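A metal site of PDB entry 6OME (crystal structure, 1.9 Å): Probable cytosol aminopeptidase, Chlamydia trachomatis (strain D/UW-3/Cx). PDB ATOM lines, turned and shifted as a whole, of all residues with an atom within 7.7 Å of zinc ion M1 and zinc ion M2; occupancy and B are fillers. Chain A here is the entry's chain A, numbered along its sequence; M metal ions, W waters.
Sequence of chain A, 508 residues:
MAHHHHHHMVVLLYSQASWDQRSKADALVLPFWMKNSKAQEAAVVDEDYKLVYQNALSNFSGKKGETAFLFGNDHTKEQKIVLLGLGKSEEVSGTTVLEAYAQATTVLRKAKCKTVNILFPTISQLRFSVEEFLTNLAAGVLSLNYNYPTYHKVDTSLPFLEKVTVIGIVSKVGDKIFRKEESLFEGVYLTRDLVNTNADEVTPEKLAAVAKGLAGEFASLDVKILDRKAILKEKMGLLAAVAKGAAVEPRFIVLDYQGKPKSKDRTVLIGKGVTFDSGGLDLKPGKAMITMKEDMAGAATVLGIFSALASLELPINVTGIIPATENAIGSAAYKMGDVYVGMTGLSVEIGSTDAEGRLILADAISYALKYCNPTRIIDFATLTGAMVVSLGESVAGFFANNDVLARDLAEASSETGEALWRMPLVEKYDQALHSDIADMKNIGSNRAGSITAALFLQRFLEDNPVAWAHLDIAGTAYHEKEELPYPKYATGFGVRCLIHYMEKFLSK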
ATOM      1  N   LYS A 272      -7.552  35.003 -16.397  1.00  0.00           N
ATOM      2  CA  LYS A 272      -7.251  33.639 -15.952  1.00  0.00           C
ATOM      3  C   LYS A 272      -8.341  32.678 -16.420  1.00  0.00           C
ATOM      4  O   LYS A 272      -9.515  32.851 -16.081  1.00  0.00           O
ATOM      5  CB  LYS A 272      -7.123  33.615 -14.429  1.00  0.00           C
ATOM      6  CG  LYS A 272      -7.099  32.194 -13.842  1.00  0.00           C
ATOM      7  CD  LYS A 272      -7.056  32.182 -12.295  1.00  0.00           C
ATOM      8  CE  LYS A 272      -7.289  30.728 -11.752  1.00  0.00           C
ATOM      9  NZ  LYS A 272      -7.164  30.610 -10.263  1.00  0.00           N
ATOM     10  N   GLY A 273      -7.956  31.682 -17.211  1.00  0.00           N
ATOM     11  CA  GLY A 273      -8.918  30.722 -17.723  1.00  0.00           C
ATOM     12  C   GLY A 273      -8.726  29.294 -17.232  1.00  0.00           C
ATOM     13  O   GLY A 273      -8.571  28.384 -18.048  1.00  0.00           O
ATOM     14  N   VAL A 274      -8.752  29.071 -15.927  1.00  0.00           N
ATOM     15  CA  VAL A 274      -8.686  27.698 -15.412  1.00  0.00           C
ATOM     16  C   VAL A 274     -10.097  27.145 -15.441  1.00  0.00           C
ATOM     17  O   VAL A 274     -10.945  27.536 -14.638  1.00  0.00           O
ATOM     18  CB  VAL A 274      -8.081  27.636 -14.009  1.00  0.00           C
ATOM     19  CG1 VAL A 274      -8.163  26.208 -13.459  1.00  0.00           C
ATOM     20  CG2 VAL A 274      -6.602  28.070 -14.079  1.00  0.00           C
ATOM     21  N   THR A 275     -10.373  26.271 -16.407  1.00  0.00           N
ATOM     22  CA  THR A 275     -11.763  25.919 -16.689  1.00  0.00           C
ATOM     23  C   THR A 275     -12.331  24.982 -15.627  1.00  0.00           C
ATOM     24  O   THR A 275     -13.558  24.879 -15.504  1.00  0.00           O
ATOM     25  CB  THR A 275     -11.877  25.309 -18.087  1.00  0.00           C
ATOM     26  OG1 THR A 275     -10.955  24.218 -18.211  1.00  0.00           O
ATOM     27  CG2 THR A 275     -11.533  26.371 -19.154  1.00  0.00           C
ATOM     28  N   PHE A 276     -11.472  24.317 -14.856  1.00  0.00           N
ATOM     29  CA  PHE A 276     -11.889  23.671 -13.618  1.00  0.00           C
ATOM     30  C   PHE A 276     -10.633  23.508 -12.762  1.00  0.00           C
ATOM     31  O   PHE A 276      -9.613  23.030 -13.252  1.00  0.00           O
ATOM     32  CB  PHE A 276     -12.548  22.300 -13.857  1.00  0.00           C
ATOM     33  CG  PHE A 276     -13.071  21.647 -12.592  1.00  0.00           C
ATOM     34  CD1 PHE A 276     -14.336  21.973 -12.084  1.00  0.00           C
ATOM     35  CD2 PHE A 276     -12.290  20.731 -11.891  1.00  0.00           C
ATOM     36  CE1 PHE A 276     -14.814  21.384 -10.906  1.00  0.00           C
ATOM     37  CE2 PHE A 276     -12.758  20.142 -10.712  1.00  0.00           C
ATOM     38  CZ  PHE A 276     -14.020  20.462 -10.223  1.00  0.00           C
ATOM     39  N   ASP A 277     -10.717  23.905 -11.500  1.00  0.00           N
ATOM     40  CA  ASP A 277      -9.595  23.886 -10.576  1.00  0.00           C
ATOM     41  C   ASP A 277      -9.839  22.831  -9.505  1.00  0.00           C
ATOM     42  O   ASP A 277     -10.562  23.080  -8.537  1.00  0.00           O
ATOM     43  CB  ASP A 277      -9.401  25.274  -9.985  1.00  0.00           C
ATOM     44  CG  ASP A 277      -8.113  25.409  -9.212  1.00  0.00           C
ATOM     45  OD1 ASP A 277      -7.323  24.442  -9.100  1.00  0.00           O
ATOM     46  OD2 ASP A 277      -7.885  26.524  -8.749  1.00  0.00           O
ATOM     47  N   SER A 278      -9.254  21.636  -9.674  1.00  0.00           N
ATOM     48  CA  SER A 278      -9.271  20.628  -8.621  1.00  0.00           C
ATOM     49  C   SER A 278      -8.309  20.967  -7.490  1.00  0.00           C
ATOM     50  O   SER A 278      -8.405  20.359  -6.412  1.00  0.00           O
ATOM     51  CB  SER A 278      -8.886  19.251  -9.159  1.00  0.00           C
ATOM     52  OG  SER A 278      -7.506  19.269  -9.526  1.00  0.00           O
ATOM     53  N   GLY A 279      -7.374  21.878  -7.725  1.00  0.00           N
ATOM     54  CA  GLY A 279      -6.258  22.122  -6.835  1.00  0.00           C
ATOM     55  C   GLY A 279      -4.989  21.390  -7.231  1.00  0.00           C
ATOM     56  O   GLY A 279      -3.903  21.760  -6.771  1.00  0.00           O
ATOM     57  N   GLY A 280      -5.088  20.371  -8.097  1.00  0.00           N
ATOM     58  CA  GLY A 280      -3.927  19.552  -8.451  1.00  0.00           C
ATOM     59  C   GLY A 280      -3.588  18.576  -7.348  1.00  0.00           C
ATOM     60  O   GLY A 280      -4.424  18.205  -6.527  1.00  0.00           O
ATOM     61  N   ASP A 282      -2.131  19.118  -4.653  1.00  0.00           N
ATOM     62  CA  ASP A 282      -2.627  19.765  -3.425  1.00  0.00           C
ATOM     63  C   ASP A 282      -4.143  19.898  -3.526  1.00  0.00           C
ATOM     64  O   ASP A 282      -4.708  20.988  -3.650  1.00  0.00           O
ATOM     65  CB  ASP A 282      -1.958  21.126  -3.245  1.00  0.00           C
ATOM     66  CG  ASP A 282      -2.110  21.680  -1.832  1.00  0.00           C
ATOM     67  OD1 ASP A 282      -2.685  20.972  -0.973  1.00  0.00           O
ATOM     68  OD2 ASP A 282      -1.655  22.814  -1.571  1.00  0.00           O
ATOM     69  N   LYS A 284      -8.063  20.159  -3.505  1.00  0.00           N
ATOM     70  CA  LYS A 284      -9.015  20.932  -2.706  1.00  0.00           C
ATOM     71  C   LYS A 284      -9.958  20.000  -1.944  1.00  0.00           C
ATOM     72  O   LYS A 284     -10.341  18.941  -2.452  1.00  0.00           O
ATOM     73  CB  LYS A 284      -9.854  21.839  -3.606  1.00  0.00           C
ATOM     74  CG  LYS A 284      -9.127  23.011  -4.239  1.00  0.00           C
ATOM     75  CD  LYS A 284     -10.138  23.781  -5.133  1.00  0.00           C
ATOM     76  CE  LYS A 284      -9.485  24.994  -5.813  1.00  0.00           C
ATOM     77  NZ  LYS A 284      -8.920  25.937  -4.821  1.00  0.00           N
ATOM     78  N   MET A 292     -15.881  25.218  -8.668  1.00  0.00           N
ATOM     79  CA  MET A 292     -14.650  25.598  -9.370  1.00  0.00           C
ATOM     80  C   MET A 292     -14.768  25.590 -10.891  1.00  0.00           C
ATOM     81  O   MET A 292     -13.753  25.842 -11.567  1.00  0.00           O
ATOM     82  CB  MET A 292     -13.492  24.723  -8.917  1.00  0.00           C
ATOM     83  CG  MET A 292     -12.956  25.147  -7.546  1.00  0.00           C
ATOM     84  SD  MET A 292     -12.324  26.848  -7.526  1.00  0.00           S
ATOM     85  CE  MET A 292     -13.631  27.708  -6.667  1.00  0.00           C
ATOM     86  N   GLU A 294     -16.078  28.072 -11.833  1.00  0.00           N
ATOM     87  CA  GLU A 294     -15.969  29.531 -11.888  1.00  0.00           C
ATOM     88  C   GLU A 294     -14.549  30.010 -12.089  1.00  0.00           C
ATOM     89  O   GLU A 294     -14.332  31.219 -12.288  1.00  0.00           O
ATOM     90  CB  GLU A 294     -16.514  30.155 -10.607  1.00  0.00           C
ATOM     91  CG  GLU A 294     -15.585  29.980  -9.378  1.00  0.00           C
ATOM     92  CD  GLU A 294     -16.032  30.836  -8.210  1.00  0.00           C
ATOM     93  OE1 GLU A 294     -15.763  32.056  -8.234  1.00  0.00           O
ATOM     94  OE2 GLU A 294     -16.698  30.317  -7.302  1.00  0.00           O
ATOM     95  N   ASP A 295     -13.566  29.108 -12.041  1.00  0.00           N
ATOM     96  CA  ASP A 295     -12.183  29.563 -11.963  1.00  0.00           C
ATOM     97  C   ASP A 295     -11.668  30.090 -13.296  1.00  0.00           C
ATOM     98  O   ASP A 295     -10.502  30.484 -13.374  1.00  0.00           O
ATOM     99  CB  ASP A 295     -11.297  28.412 -11.456  1.00  0.00           C
ATOM    100  CG  ASP A 295     -10.083  28.910 -10.675  1.00  0.00           C
ATOM    101  OD1 ASP A 295     -10.171  29.941  -9.962  1.00  0.00           O
ATOM    102  OD2 ASP A 295      -9.035  28.247 -10.790  1.00  0.00           O
ATOM    103  N   MET A 296     -12.519  30.125 -14.327  1.00  0.00           N
ATOM    104  CA  MET A 296     -12.177  30.742 -15.601  1.00  0.00           C
ATOM    105  C   MET A 296     -12.898  32.065 -15.774  1.00  0.00           C
ATOM    106  O   MET A 296     -12.966  32.592 -16.897  1.00  0.00           O
ATOM    107  CB  MET A 296     -12.458  29.791 -16.777  1.00  0.00           C
ATOM    108  CG  MET A 296     -13.764  28.985 -16.694  1.00  0.00           C
ATOM    109  SD  MET A 296     -15.271  29.982 -16.522  1.00  0.00           S
ATOM    110  CE  MET A 296     -15.392  30.686 -18.181  1.00  0.00           C
ATOM    111  N   ASN A 327      -6.900  22.509 -14.162  1.00  0.00           N
ATOM    112  CA  ASN A 327      -5.881  22.175 -13.153  1.00  0.00           C
ATOM    113  C   ASN A 327      -6.315  20.838 -12.565  1.00  0.00           C
ATOM    114  O   ASN A 327      -7.129  20.760 -11.645  1.00  0.00           O
ATOM    115  CB  ASN A 327      -5.780  23.245 -12.058  1.00  0.00           C
ATOM    116  CG  ASN A 327      -4.563  23.018 -11.146  1.00  0.00           C
ATOM    117  OD1 ASN A 327      -3.569  22.404 -11.542  1.00  0.00           O
ATOM    118  ND2 ASN A 327      -4.633  23.530  -9.918  1.00  0.00           N
ATOM    119  N   TYR A 334       1.521  18.365 -12.491  1.00  0.00           N
ATOM    120  CA  TYR A 334       2.781  19.006 -12.112  1.00  0.00           C
ATOM    121  C   TYR A 334       2.952  18.936 -10.599  1.00  0.00           C
ATOM    122  O   TYR A 334       1.981  18.858  -9.834  1.00  0.00           O
ATOM    123  CB  TYR A 334       2.846  20.446 -12.626  1.00  0.00           C
ATOM    124  CG  TYR A 334       2.073  21.531 -11.878  1.00  0.00           C
ATOM    125  CD1 TYR A 334       0.680  21.483 -11.738  1.00  0.00           C
ATOM    126  CD2 TYR A 334       2.737  22.643 -11.361  1.00  0.00           C
ATOM    127  CE1 TYR A 334      -0.017  22.524 -11.079  1.00  0.00           C
ATOM    128  CE2 TYR A 334       2.074  23.676 -10.725  1.00  0.00           C
ATOM    129  CZ  TYR A 334       0.691  23.608 -10.578  1.00  0.00           C
ATOM    130  OH  TYR A 334       0.076  24.654  -9.927  1.00  0.00           O
ATOM    131  N   SER A 352       2.524  25.272  -3.729  1.00  0.00           N
ATOM    132  CA  SER A 352       1.215  24.622  -3.815  1.00  0.00           C
ATOM    133  C   SER A 352       0.749  24.582  -5.257  1.00  0.00           C
ATOM    134  O   SER A 352       0.735  25.602  -5.946  1.00  0.00           O
ATOM    135  CB  SER A 352       0.153  25.352  -2.968  1.00  0.00           C
ATOM    136  OG  SER A 352      -1.141  24.812  -3.268  1.00  0.00           O
ATOM    137  N   THR A 353       0.360  23.390  -5.722  1.00  0.00           N
ATOM    138  CA  THR A 353      -0.226  23.284  -7.057  1.00  0.00           C
ATOM    139  C   THR A 353      -1.583  23.988  -7.157  1.00  0.00           C
ATOM    140  O   THR A 353      -2.074  24.176  -8.284  1.00  0.00           O
ATOM    141  CB  THR A 353      -0.382  21.822  -7.446  1.00  0.00           C
ATOM    142  OG1 THR A 353      -1.282  21.190  -6.530  1.00  0.00           O
ATOM    143  CG2 THR A 353       0.977  21.097  -7.413  1.00  0.00           C
ATOM    144  N   ASP A 354      -2.211  24.334  -6.035  1.00  0.00           N
ATOM    145  CA  ASP A 354      -3.466  25.088  -6.028  1.00  0.00           C
ATOM    146  C   ASP A 354      -3.233  26.584  -6.212  1.00  0.00           C
ATOM    147  O   ASP A 354      -4.201  27.350  -6.224  1.00  0.00           O
ATOM    148  CB  ASP A 354      -4.232  24.805  -4.723  1.00  0.00           C
ATOM    149  CG  ASP A 354      -5.741  25.121  -4.808  1.00  0.00           C
ATOM    150  OD1 ASP A 354      -6.286  25.276  -5.912  1.00  0.00           O
ATOM    151  OD2 ASP A 354      -6.397  25.186  -3.748  1.00  0.00           O
ATOM    152  N   ALA A 355      -1.989  27.032  -6.274  1.00  0.00           N
ATOM    153  CA  ALA A 355      -1.687  28.411  -6.684  1.00  0.00           C
ATOM    154  C   ALA A 355      -1.276  28.426  -8.154  1.00  0.00           C
ATOM    155  O   ALA A 355      -0.185  28.881  -8.511  1.00  0.00           O
ATOM    156  CB  ALA A 355      -0.605  29.005  -5.787  1.00  0.00           C
ATOM    157  N   GLU A 356      -2.143  27.868  -9.005  1.00  0.00           N
ATOM    158  CA  GLU A 356      -1.853  27.648 -10.408  1.00  0.00           C
ATOM    159  C   GLU A 356      -2.222  28.847 -11.280  1.00  0.00           C
ATOM    160  O   GLU A 356      -1.621  29.041 -12.328  1.00  0.00           O
ATOM    161  CB  GLU A 356      -2.597  26.390 -10.933  1.00  0.00           C
ATOM    162  CG  GLU A 356      -4.039  26.662 -11.472  1.00  0.00           C
ATOM    163  CD  GLU A 356      -5.015  27.145 -10.401  1.00  0.00           C
ATOM    164  OE1 GLU A 356      -4.749  26.885  -9.204  1.00  0.00           O
ATOM    165  OE2 GLU A 356      -6.071  27.774 -10.724  1.00  0.00           O
ATOM    166  N   GLY A 357      -3.213  29.638 -10.856  1.00  0.00           N
ATOM    167  CA  GLY A 357      -3.656  30.732 -11.706  1.00  0.00           C
ATOM    168  C   GLY A 357      -2.574  31.771 -11.915  1.00  0.00           C
ATOM    169  O   GLY A 357      -2.402  32.293 -13.016  1.00  0.00           O
ATOM    170  N   ARG A 358      -1.802  32.063 -10.855  1.00  0.00           N
ATOM    171  CA  ARG A 358      -0.752  33.064 -10.992  1.00  0.00           C
ATOM    172  C   ARG A 358       0.336  32.582 -11.948  1.00  0.00           C
ATOM    173  O   ARG A 358       0.971  33.399 -12.619  1.00  0.00           O
ATOM    174  CB  ARG A 358      -0.156  33.394  -9.612  1.00  0.00           C
ATOM    175  CG  ARG A 358       0.570  32.253  -8.932  1.00  0.00           C
ATOM    176  CD  ARG A 358       0.761  32.566  -7.435  1.00  0.00           C
ATOM    177  NE  ARG A 358      -0.529  32.463  -6.759  1.00  0.00           N
ATOM    178  CZ  ARG A 358      -0.709  32.717  -5.465  1.00  0.00           C
ATOM    179  NH1 ARG A 358       0.318  33.087  -4.718  1.00  0.00           N
ATOM    180  NH2 ARG A 358      -1.925  32.610  -4.924  1.00  0.00           N
ATOM    181  N   ILE A 360      -0.159  30.698 -14.753  1.00  0.00           N
ATOM    182  CA  ILE A 360      -0.533  30.867 -16.152  1.00  0.00           C
ATOM    183  C   ILE A 360      -0.649  32.340 -16.495  1.00  0.00           C
ATOM    184  O   ILE A 360      -0.398  32.740 -17.638  1.00  0.00           O
ATOM    185  CB  ILE A 360      -1.808  30.071 -16.493  1.00  0.00           C
ATOM    186  CG1 ILE A 360      -3.075  30.764 -15.989  1.00  0.00           C
ATOM    187  CG2 ILE A 360      -1.752  28.644 -15.920  1.00  0.00           C
ATOM    188  CD1 ILE A 360      -4.332  29.971 -16.317  1.00  0.00           C
ATOM    189  N   THR A 382      -9.953  34.990 -10.705  1.00  0.00           N
ATOM    190  CA  THR A 382     -10.453  34.403  -9.458  1.00  0.00           C
ATOM    191  C   THR A 382      -9.252  33.801  -8.735  1.00  0.00           C
ATOM    192  O   THR A 382      -9.004  32.593  -8.765  1.00  0.00           O
ATOM    193  CB  THR A 382     -11.514  33.355  -9.733  1.00  0.00           C
ATOM    194  OG1 THR A 382     -11.005  32.438 -10.721  1.00  0.00           O
ATOM    195  CG2 THR A 382     -12.812  33.977 -10.245  1.00  0.00           C
ATOM    196  N   LEU A 383      -8.463  34.660  -8.103  1.00  0.00           N
ATOM    197  CA  LEU A 383      -7.118  34.246  -7.758  1.00  0.00           C
ATOM    198  C   LEU A 383      -6.987  33.683  -6.346  1.00  0.00           C
ATOM    199  O   LEU A 383      -6.390  32.618  -6.172  1.00  0.00           O
ATOM    200  CB  LEU A 383      -6.121  35.411  -7.948  1.00  0.00           C
ATOM    201  CG  LEU A 383      -4.677  34.948  -8.135  1.00  0.00           C
ATOM    202  CD1 LEU A 383      -4.573  34.054  -9.370  1.00  0.00           C
ATOM    203  CD2 LEU A 383      -3.693  36.128  -8.246  1.00  0.00           C
ATOM    204  N   THR A 384      -7.483  34.375  -5.304  1.00  0.00           N
ATOM    205  CA  THR A 384      -7.150  33.931  -3.950  1.00  0.00           C
ATOM    206  C   THR A 384      -8.358  33.869  -3.038  1.00  0.00           C
ATOM    207  O   THR A 384      -9.190  34.785  -3.022  1.00  0.00           O
ATOM    208  CB  THR A 384      -6.084  34.853  -3.280  1.00  0.00           C
ATOM    209  OG1 THR A 384      -6.596  36.198  -3.190  1.00  0.00           O
ATOM    210  CG2 THR A 384      -4.789  34.855  -4.104  1.00  0.00           C
HETATM  211 ZN    ZN M   1      -7.441  28.585  -9.732  1.00  0.00          ZN
HETATM  212 ZN    ZN M   2      -6.127  26.875  -7.528  1.00  0.00          ZN
HETATM  213  O   HOH W   1      -6.811  29.066  -7.841  1.00  0.00           O
HETATM  214  O   HOH W   2      -8.497  28.705  -6.125  1.00  0.00           O
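N of Gly 279 lies within hydrogen-bond range of OD1 of Asp 277, at 2.9 Å.
N of Asp 354 lies within hydrogen-bond range of OG of Ser 352, 3.0 Å away.
The side-chain carboxylate (OD2) of Asp 354 is in salt-bridge range of the side-chain amino group (NZ) of Lys 284, at 2.8 Å.
The side-chain hydroxyl of Thr 382 sits at hydrogen-bond distance from the side-chain carboxylate of Asp 295, 2.7 Å away.
ND2 of Asn 327 sits close to OE1 of Glu 356 (3.4 Å).
The backbone carbonyl oxygen (O) of Thr 382 sits close to the side-chain amino group (NZ) of Lys 272 (3.1 Å).
The backbone NH of Asp 354 lies within hydrogen-bond range of the backbone carbonyl oxygen of Gly 279.
The backbone NH (N) of Val 274 sits at hydrogen-bond distance from the backbone carbonyl oxygen (O) of Asp 295, at 3.4 Å.
Within 4 Å of zinc ion M1: Lys 272, Asp 277, Asp 295 and Glu 356.
Of the 28 residues printed, 3 come within 4 Å of zinc ion M2.
Zinc ion M1 is bound by the side-chain carboxylate of Glu 356, the side-chain carboxylate of Asp 295, water W1, the side-chain amino group of Lys 272 and the side-chain carboxylate of Asp 277.
Zinc ion M1 has five donor atoms within binding distance.
The side-chain carboxylate (OD2) of Asp 277 is bound to zinc ion M2 (2.2 Å).
The side-chain carboxylate (OE1) of Glu 356 binds zinc ion M2 (2.2 Å).
OD1 of Asp 354 is bound to zinc ion M2 (2.3 Å).
Water W1 binds zinc ion M2 (2.3 Å).
Zinc ion M2 is bound by O of Asp 354, at 2.4 Å.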
